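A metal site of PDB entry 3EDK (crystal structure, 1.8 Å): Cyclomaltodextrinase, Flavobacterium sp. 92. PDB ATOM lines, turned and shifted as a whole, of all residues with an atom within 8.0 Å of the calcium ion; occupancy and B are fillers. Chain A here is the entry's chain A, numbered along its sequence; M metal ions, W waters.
The side-chain hydroxyl (OG) of Ser 222 is bound to the calcium ion (2.3 Å). O of Tyr 315 is bound to the calcium ion, at 2.4 Å. The calcium ion is bound by water W1, 2.4 Å away. Water W2 is bound to the calcium ion, 2.4 Å away. The calcium ion is bound by the backbone carbonyl oxygen (O) of Thr 270 (2.4 Å). OD2 of Asp 280 binds the calcium ion (2.5 Å). OD1 of Asp 280 binds the calcium ion, at 2.5 Å. The calcium ion has seven donor atoms within binding distance.
Within 4 Å of the calcium ion: Ser 222, Thr 270, Asp 280 and Tyr 315. The nearest printed residue that does not touch the calcium ion is Lys 271 (4.2 Å).
N of Ser 222 sits at hydrogen-bond distance from OG of Ser 316 (3.4 Å). The backbone carbonyl oxygen (O) of Ser 222 sits at hydrogen-bond distance from the backbone NH (N) of Leu 281, 2.7 Å away. O of Asp 280 lies within hydrogen-bond range of N of Asn 241, at 2.8 Å.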
ATOM      1  N   LEU A 221      36.428  12.854 -29.742  1.00  0.00           N
ATOM      2  CA  LEU A 221      36.575  13.727 -28.587  1.00  0.00           C
ATOM      3  C   LEU A 221      35.647  13.332 -27.446  1.00  0.00           C
ATOM      4  O   LEU A 221      36.026  13.439 -26.281  1.00  0.00           O
ATOM      5  CB  LEU A 221      36.298  15.181 -28.983  1.00  0.00           C
ATOM      6  CG  LEU A 221      37.210  15.779 -30.076  1.00  0.00           C
ATOM      7  CD1 LEU A 221      36.785  17.217 -30.317  1.00  0.00           C
ATOM      8  CD2 LEU A 221      38.675  15.693 -29.643  1.00  0.00           C
ATOM      9  N   SER A 222      34.434  12.900 -27.805  1.00  0.00           N
ATOM     10  CA  SER A 222      33.380  12.591 -26.835  1.00  0.00           C
ATOM     11  C   SER A 222      33.599  11.323 -25.981  1.00  0.00           C
ATOM     12  O   SER A 222      33.215  11.281 -24.795  1.00  0.00           O
ATOM     13  CB  SER A 222      32.032  12.523 -27.580  1.00  0.00           C
ATOM     14  OG  SER A 222      30.975  12.229 -26.702  1.00  0.00           O
ATOM     15  N   HIS A 223      34.192  10.310 -26.591  1.00  0.00           N
ATOM     16  CA  HIS A 223      34.301   8.992 -25.949  1.00  0.00           C
ATOM     17  C   HIS A 223      35.606   8.261 -26.195  1.00  0.00           C
ATOM     18  O   HIS A 223      36.418   8.605 -27.071  1.00  0.00           O
ATOM     19  CB  HIS A 223      33.121   8.091 -26.389  1.00  0.00           C
ATOM     20  CG  HIS A 223      33.057   7.835 -27.864  1.00  0.00           C
ATOM     21  ND1 HIS A 223      32.329   8.618 -28.727  1.00  0.00           N
ATOM     22  CD2 HIS A 223      33.671   6.907 -28.639  1.00  0.00           C
ATOM     23  CE1 HIS A 223      32.443   8.164 -29.957  1.00  0.00           C
ATOM     24  NE2 HIS A 223      33.263   7.133 -29.935  1.00  0.00           N
ATOM     25  N   ASN A 241      31.752  10.668 -17.610  1.00  0.00           N
ATOM     26  CA  ASN A 241      30.410  11.060 -17.244  1.00  0.00           C
ATOM     27  C   ASN A 241      29.654   9.931 -16.520  1.00  0.00           C
ATOM     28  O   ASN A 241      29.874   8.751 -16.800  1.00  0.00           O
ATOM     29  CB  ASN A 241      29.651  11.524 -18.480  1.00  0.00           C
ATOM     30  CG  ASN A 241      30.078  12.922 -18.907  1.00  0.00           C
ATOM     31  OD1 ASN A 241      30.386  13.172 -20.092  1.00  0.00           O
ATOM     32  ND2 ASN A 241      30.122  13.841 -17.968  1.00  0.00           N
ATOM     33  N   THR A 249      23.161   7.555 -24.015  1.00  0.00           N
ATOM     34  CA  THR A 249      22.485   8.644 -24.718  1.00  0.00           C
ATOM     35  C   THR A 249      21.287   8.123 -25.528  1.00  0.00           C
ATOM     36  O   THR A 249      21.303   6.985 -26.064  1.00  0.00           O
ATOM     37  CB  THR A 249      23.434   9.435 -25.672  1.00  0.00           C
ATOM     38  OG1 THR A 249      22.724  10.578 -26.145  1.00  0.00           O
ATOM     39  CG2 THR A 249      23.882   8.579 -26.886  1.00  0.00           C
ATOM     40  N   GLU A 267      21.951  17.465 -21.629  1.00  0.00           N
ATOM     41  CA  GLU A 267      22.909  16.699 -20.864  1.00  0.00           C
ATOM     42  C   GLU A 267      22.983  15.268 -21.357  1.00  0.00           C
ATOM     43  O   GLU A 267      24.066  14.715 -21.500  1.00  0.00           O
ATOM     44  CB  GLU A 267      22.560  16.780 -19.373  1.00  0.00           C
ATOM     45  CG  GLU A 267      22.662  18.179 -18.834  1.00  0.00           C
ATOM     46  CD  GLU A 267      24.094  18.650 -18.753  1.00  0.00           C
ATOM     47  OE1 GLU A 267      24.441  19.618 -19.459  1.00  0.00           O
ATOM     48  OE2 GLU A 267      24.887  18.002 -18.030  1.00  0.00           O
ATOM     49  N   ASN A 268      21.833  14.667 -21.646  1.00  0.00           N
ATOM     50  CA  ASN A 268      21.844  13.308 -22.110  1.00  0.00           C
ATOM     51  C   ASN A 268      22.595  13.187 -23.433  1.00  0.00           C
ATOM     52  O   ASN A 268      23.212  12.173 -23.697  1.00  0.00           O
ATOM     53  CB  ASN A 268      20.425  12.717 -22.232  1.00  0.00           C
ATOM     54  CG  ASN A 268      20.449  11.306 -22.783  1.00  0.00           C
ATOM     55  OD1 ASN A 268      20.204  11.116 -23.964  1.00  0.00           O
ATOM     56  ND2 ASN A 268      20.761  10.309 -21.936  1.00  0.00           N
ATOM     57  N   PHE A 269      22.507  14.214 -24.259  1.00  0.00           N
ATOM     58  CA  PHE A 269      23.177  14.178 -25.553  1.00  0.00           C
ATOM     59  C   PHE A 269      24.695  14.283 -25.402  1.00  0.00           C
ATOM     60  O   PHE A 269      25.440  13.553 -26.040  1.00  0.00           O
ATOM     61  CB  PHE A 269      22.685  15.260 -26.494  1.00  0.00           C
ATOM     62  CG  PHE A 269      23.148  15.051 -27.910  1.00  0.00           C
ATOM     63  CD1 PHE A 269      22.765  13.889 -28.598  1.00  0.00           C
ATOM     64  CD2 PHE A 269      23.992  15.976 -28.547  1.00  0.00           C
ATOM     65  CE1 PHE A 269      23.194  13.632 -29.922  1.00  0.00           C
ATOM     66  CE2 PHE A 269      24.409  15.720 -29.898  1.00  0.00           C
ATOM     67  CZ  PHE A 269      24.014  14.534 -30.553  1.00  0.00           C
ATOM     68  N   THR A 270      25.148  15.207 -24.559  1.00  0.00           N
ATOM     69  CA  THR A 270      26.577  15.498 -24.427  1.00  0.00           C
ATOM     70  C   THR A 270      27.306  14.635 -23.389  1.00  0.00           C
ATOM     71  O   THR A 270      28.522  14.537 -23.445  1.00  0.00           O
ATOM     72  CB  THR A 270      26.861  17.003 -24.118  1.00  0.00           C
ATOM     73  OG1 THR A 270      26.363  17.331 -22.807  1.00  0.00           O
ATOM     74  CG2 THR A 270      26.252  17.970 -25.176  1.00  0.00           C
ATOM     75  N   LYS A 271      26.560  14.052 -22.435  1.00  0.00           N
ATOM     76  CA  LYS A 271      27.131  13.189 -21.377  1.00  0.00           C
ATOM     77  C   LYS A 271      26.780  11.719 -21.507  1.00  0.00           C
ATOM     78  O   LYS A 271      27.538  10.856 -21.036  1.00  0.00           O
ATOM     79  CB  LYS A 271      26.752  13.680 -19.963  1.00  0.00           C
ATOM     80  CG  LYS A 271      27.322  15.048 -19.618  1.00  0.00           C
ATOM     81  CD  LYS A 271      27.113  15.402 -18.107  1.00  0.00           C
ATOM     82  CE  LYS A 271      28.029  16.540 -17.655  1.00  0.00           C
ATOM     83  NZ  LYS A 271      27.667  17.785 -18.376  1.00  0.00           N
ATOM     84  N   GLY A 272      25.634  11.431 -22.119  1.00  0.00           N
ATOM     85  CA  GLY A 272      25.205  10.047 -22.340  1.00  0.00           C
ATOM     86  C   GLY A 272      26.212   9.217 -23.133  1.00  0.00           C
ATOM     87  O   GLY A 272      26.839   9.706 -24.089  1.00  0.00           O
ATOM     88  N   TRP A 273      26.378   7.956 -22.749  1.00  0.00           N
ATOM     89  CA  TRP A 273      27.332   7.082 -23.426  1.00  0.00           C
ATOM     90  C   TRP A 273      26.804   6.648 -24.790  1.00  0.00           C
ATOM     91  O   TRP A 273      25.664   6.204 -24.938  1.00  0.00           O
ATOM     92  CB  TRP A 273      27.624   5.849 -22.574  1.00  0.00           C
ATOM     93  CG  TRP A 273      28.405   6.069 -21.346  1.00  0.00           C
ATOM     94  CD1 TRP A 273      28.411   7.178 -20.519  1.00  0.00           C
ATOM     95  CD2 TRP A 273      29.255   5.120 -20.732  1.00  0.00           C
ATOM     96  NE1 TRP A 273      29.230   6.959 -19.440  1.00  0.00           N
ATOM     97  CE2 TRP A 273      29.760   5.694 -19.543  1.00  0.00           C
ATOM     98  CE3 TRP A 273      29.646   3.813 -21.082  1.00  0.00           C
ATOM     99  CZ2 TRP A 273      30.658   5.021 -18.703  1.00  0.00           C
ATOM    100  CZ3 TRP A 273      30.531   3.137 -20.239  1.00  0.00           C
ATOM    101  CH2 TRP A 273      31.016   3.758 -19.066  1.00  0.00           C
ATOM    102  N   PHE A 274      27.658   6.746 -25.796  1.00  0.00           N
ATOM    103  CA  PHE A 274      27.240   6.423 -27.146  1.00  0.00           C
ATOM    104  C   PHE A 274      26.688   4.983 -27.204  1.00  0.00           C
ATOM    105  O   PHE A 274      25.569   4.745 -27.714  1.00  0.00           O
ATOM    106  CB  PHE A 274      28.383   6.614 -28.143  1.00  0.00           C
ATOM    107  CG  PHE A 274      27.907   6.700 -29.558  1.00  0.00           C
ATOM    108  CD1 PHE A 274      27.959   5.587 -30.392  1.00  0.00           C
ATOM    109  CD2 PHE A 274      27.333   7.880 -30.044  1.00  0.00           C
ATOM    110  CE1 PHE A 274      27.482   5.652 -31.709  1.00  0.00           C
ATOM    111  CE2 PHE A 274      26.849   7.964 -31.325  1.00  0.00           C
ATOM    112  CZ  PHE A 274      26.929   6.844 -32.179  1.00  0.00           C
ATOM    113  N   MET A 278      31.619   2.368 -24.958  1.00  0.00           N
ATOM    114  CA  MET A 278      32.259   3.682 -25.225  1.00  0.00           C
ATOM    115  C   MET A 278      32.044   4.704 -24.107  1.00  0.00           C
ATOM    116  O   MET A 278      31.154   5.597 -24.211  1.00  0.00           O
ATOM    117  CB  MET A 278      31.796   4.254 -26.570  1.00  0.00           C
ATOM    118  CG  MET A 278      32.321   3.482 -27.775  1.00  0.00           C
ATOM    119  SD  MET A 278      31.550   4.154 -29.258  1.00  0.00           S
ATOM    120  CE  MET A 278      32.558   3.355 -30.515  1.00  0.00           C
ATOM    121  N   PRO A 279      32.828   4.562 -23.003  1.00  0.00           N
ATOM    122  CA  PRO A 279      32.739   5.535 -21.903  1.00  0.00           C
ATOM    123  C   PRO A 279      32.848   6.972 -22.388  1.00  0.00           C
ATOM    124  O   PRO A 279      33.707   7.300 -23.223  1.00  0.00           O
ATOM    125  CB  PRO A 279      33.962   5.197 -21.037  1.00  0.00           C
ATOM    126  CG  PRO A 279      34.208   3.728 -21.278  1.00  0.00           C
ATOM    127  CD  PRO A 279      33.799   3.494 -22.730  1.00  0.00           C
ATOM    128  N   ASP A 280      32.015   7.825 -21.808  1.00  0.00           N
ATOM    129  CA  ASP A 280      31.879   9.187 -22.277  1.00  0.00           C
ATOM    130  C   ASP A 280      32.700  10.140 -21.431  1.00  0.00           C
ATOM    131  O   ASP A 280      32.568  10.185 -20.204  1.00  0.00           O
ATOM    132  CB  ASP A 280      30.422   9.588 -22.254  1.00  0.00           C
ATOM    133  CG  ASP A 280      30.155  10.781 -23.151  1.00  0.00           C
ATOM    134  OD1 ASP A 280      30.179  11.922 -22.629  1.00  0.00           O
ATOM    135  OD2 ASP A 280      29.969  10.561 -24.369  1.00  0.00           O
ATOM    136  N   LEU A 281      33.565  10.918 -22.099  1.00  0.00           N
ATOM    137  CA  LEU A 281      34.479  11.821 -21.392  1.00  0.00           C
ATOM    138  C   LEU A 281      33.779  13.059 -20.861  1.00  0.00           C
ATOM    139  O   LEU A 281      33.054  13.729 -21.587  1.00  0.00           O
ATOM    140  CB  LEU A 281      35.658  12.230 -22.311  1.00  0.00           C
ATOM    141  CG  LEU A 281      36.528  11.118 -22.879  1.00  0.00           C
ATOM    142  CD1 LEU A 281      37.658  11.713 -23.709  1.00  0.00           C
ATOM    143  CD2 LEU A 281      37.091  10.192 -21.778  1.00  0.00           C
ATOM    144  N   ASN A 282      34.009  13.377 -19.594  1.00  0.00           N
ATOM    145  CA  ASN A 282      33.467  14.580 -19.001  1.00  0.00           C
ATOM    146  C   ASN A 282      34.282  15.818 -19.381  1.00  0.00           C
ATOM    147  O   ASN A 282      35.205  16.224 -18.667  1.00  0.00           O
ATOM    148  CB  ASN A 282      33.388  14.438 -17.466  1.00  0.00           C
ATOM    149  CG  ASN A 282      32.834  15.674 -16.809  1.00  0.00           C
ATOM    150  OD1 ASN A 282      32.276  16.549 -17.481  1.00  0.00           O
ATOM    151  ND2 ASN A 282      32.973  15.750 -15.481  1.00  0.00           N
ATOM    152  N   GLN A 283      33.909  16.444 -20.492  1.00  0.00           N
ATOM    153  CA  GLN A 283      34.687  17.568 -20.987  1.00  0.00           C
ATOM    154  C   GLN A 283      34.442  18.874 -20.221  1.00  0.00           C
ATOM    155  O   GLN A 283      35.088  19.884 -20.503  1.00  0.00           O
ATOM    156  CB  GLN A 283      34.451  17.747 -22.473  1.00  0.00           C
ATOM    157  CG  GLN A 283      34.941  16.570 -23.315  1.00  0.00           C
ATOM    158  CD  GLN A 283      34.083  16.338 -24.535  1.00  0.00           C
ATOM    159  OE1 GLN A 283      32.874  16.583 -24.514  1.00  0.00           O
ATOM    160  NE2 GLN A 283      34.700  15.896 -25.625  1.00  0.00           N
ATOM    161  N   THR A 312      31.421  12.393 -34.237  1.00  0.00           N
ATOM    162  CA  THR A 312      30.315  12.561 -33.246  1.00  0.00           C
ATOM    163  C   THR A 312      30.318  13.979 -32.699  1.00  0.00           C
ATOM    164  O   THR A 312      30.427  14.181 -31.481  1.00  0.00           O
ATOM    165  CB  THR A 312      30.438  11.510 -32.040  1.00  0.00           C
ATOM    166  OG1 THR A 312      31.805  11.287 -31.678  1.00  0.00           O
ATOM    167  CG2 THR A 312      29.817  10.157 -32.414  1.00  0.00           C
ATOM    168  N   TYR A 313      30.207  14.951 -33.611  1.00  0.00           N
ATOM    169  CA  TYR A 313      30.605  16.303 -33.258  1.00  0.00           C
ATOM    170  C   TYR A 313      29.839  16.866 -32.014  1.00  0.00           C
ATOM    171  O   TYR A 313      30.472  17.257 -31.019  1.00  0.00           O
ATOM    172  CB  TYR A 313      30.447  17.258 -34.448  1.00  0.00           C
ATOM    173  CG  TYR A 313      31.138  18.550 -34.139  1.00  0.00           C
ATOM    174  CD1 TYR A 313      32.556  18.600 -34.143  1.00  0.00           C
ATOM    175  CD2 TYR A 313      30.419  19.698 -33.769  1.00  0.00           C
ATOM    176  CE1 TYR A 313      33.209  19.762 -33.788  1.00  0.00           C
ATOM    177  CE2 TYR A 313      31.079  20.883 -33.435  1.00  0.00           C
ATOM    178  CZ  TYR A 313      32.491  20.890 -33.441  1.00  0.00           C
ATOM    179  OH  TYR A 313      33.198  22.041 -33.089  1.00  0.00           O
ATOM    180  N   GLY A 314      28.505  16.906 -32.097  1.00  0.00           N
ATOM    181  CA  GLY A 314      27.729  17.559 -31.024  1.00  0.00           C
ATOM    182  C   GLY A 314      27.589  16.755 -29.738  1.00  0.00           C
ATOM    183  O   GLY A 314      27.002  17.242 -28.766  1.00  0.00           O
ATOM    184  N   TYR A 315      28.075  15.517 -29.760  1.00  0.00           N
ATOM    185  CA  TYR A 315      28.123  14.668 -28.560  1.00  0.00           C
ATOM    186  C   TYR A 315      29.183  15.125 -27.554  1.00  0.00           C
ATOM    187  O   TYR A 315      29.240  14.603 -26.439  1.00  0.00           O
ATOM    188  CB  TYR A 315      28.373  13.224 -28.929  1.00  0.00           C
ATOM    189  CG  TYR A 315      27.288  12.533 -29.681  1.00  0.00           C
ATOM    190  CD1 TYR A 315      26.302  11.787 -28.992  1.00  0.00           C
ATOM    191  CD2 TYR A 315      27.250  12.576 -31.081  1.00  0.00           C
ATOM    192  CE1 TYR A 315      25.313  11.106 -29.682  1.00  0.00           C
ATOM    193  CE2 TYR A 315      26.248  11.895 -31.799  1.00  0.00           C
ATOM    194  CZ  TYR A 315      25.289  11.169 -31.100  1.00  0.00           C
ATOM    195  OH  TYR A 315      24.322  10.493 -31.781  1.00  0.00           O
ATOM    196  N   SER A 316      30.026  16.072 -27.933  1.00  0.00           N
ATOM    197  CA  SER A 316      30.922  16.700 -26.976  1.00  0.00           C
ATOM    198  C   SER A 316      30.238  17.892 -26.326  1.00  0.00           C
ATOM    199  O   SER A 316      29.337  18.521 -26.916  1.00  0.00           O
ATOM    200  CB  SER A 316      32.261  17.110 -27.625  1.00  0.00           C
ATOM    201  OG  SER A 316      33.015  15.960 -27.912  1.00  0.00           O
ATOM    202  N   ASP A 317      30.630  18.181 -25.093  1.00  0.00           N
ATOM    203  CA  ASP A 317      30.135  19.374 -24.397  1.00  0.00           C
ATOM    204  C   ASP A 317      30.290  20.620 -25.285  1.00  0.00           C
ATOM    205  O   ASP A 317      31.384  20.870 -25.805  1.00  0.00           O
ATOM    206  CB  ASP A 317      30.926  19.596 -23.105  1.00  0.00           C
ATOM    207  CG  ASP A 317      30.384  20.752 -22.299  1.00  0.00           C
ATOM    208  OD1 ASP A 317      30.929  21.871 -22.414  1.00  0.00           O
ATOM    209  OD2 ASP A 317      29.383  20.540 -21.596  1.00  0.00           O
HETATM  210 CA    CA M   1      29.795  12.964 -24.815  1.00  0.00          CA
HETATM  211  O   HOH W   1      27.605  12.052 -25.164  1.00  0.00           O
HETATM  212  O   HOH W   2      31.667  14.244 -23.950  1.00  0.00           O
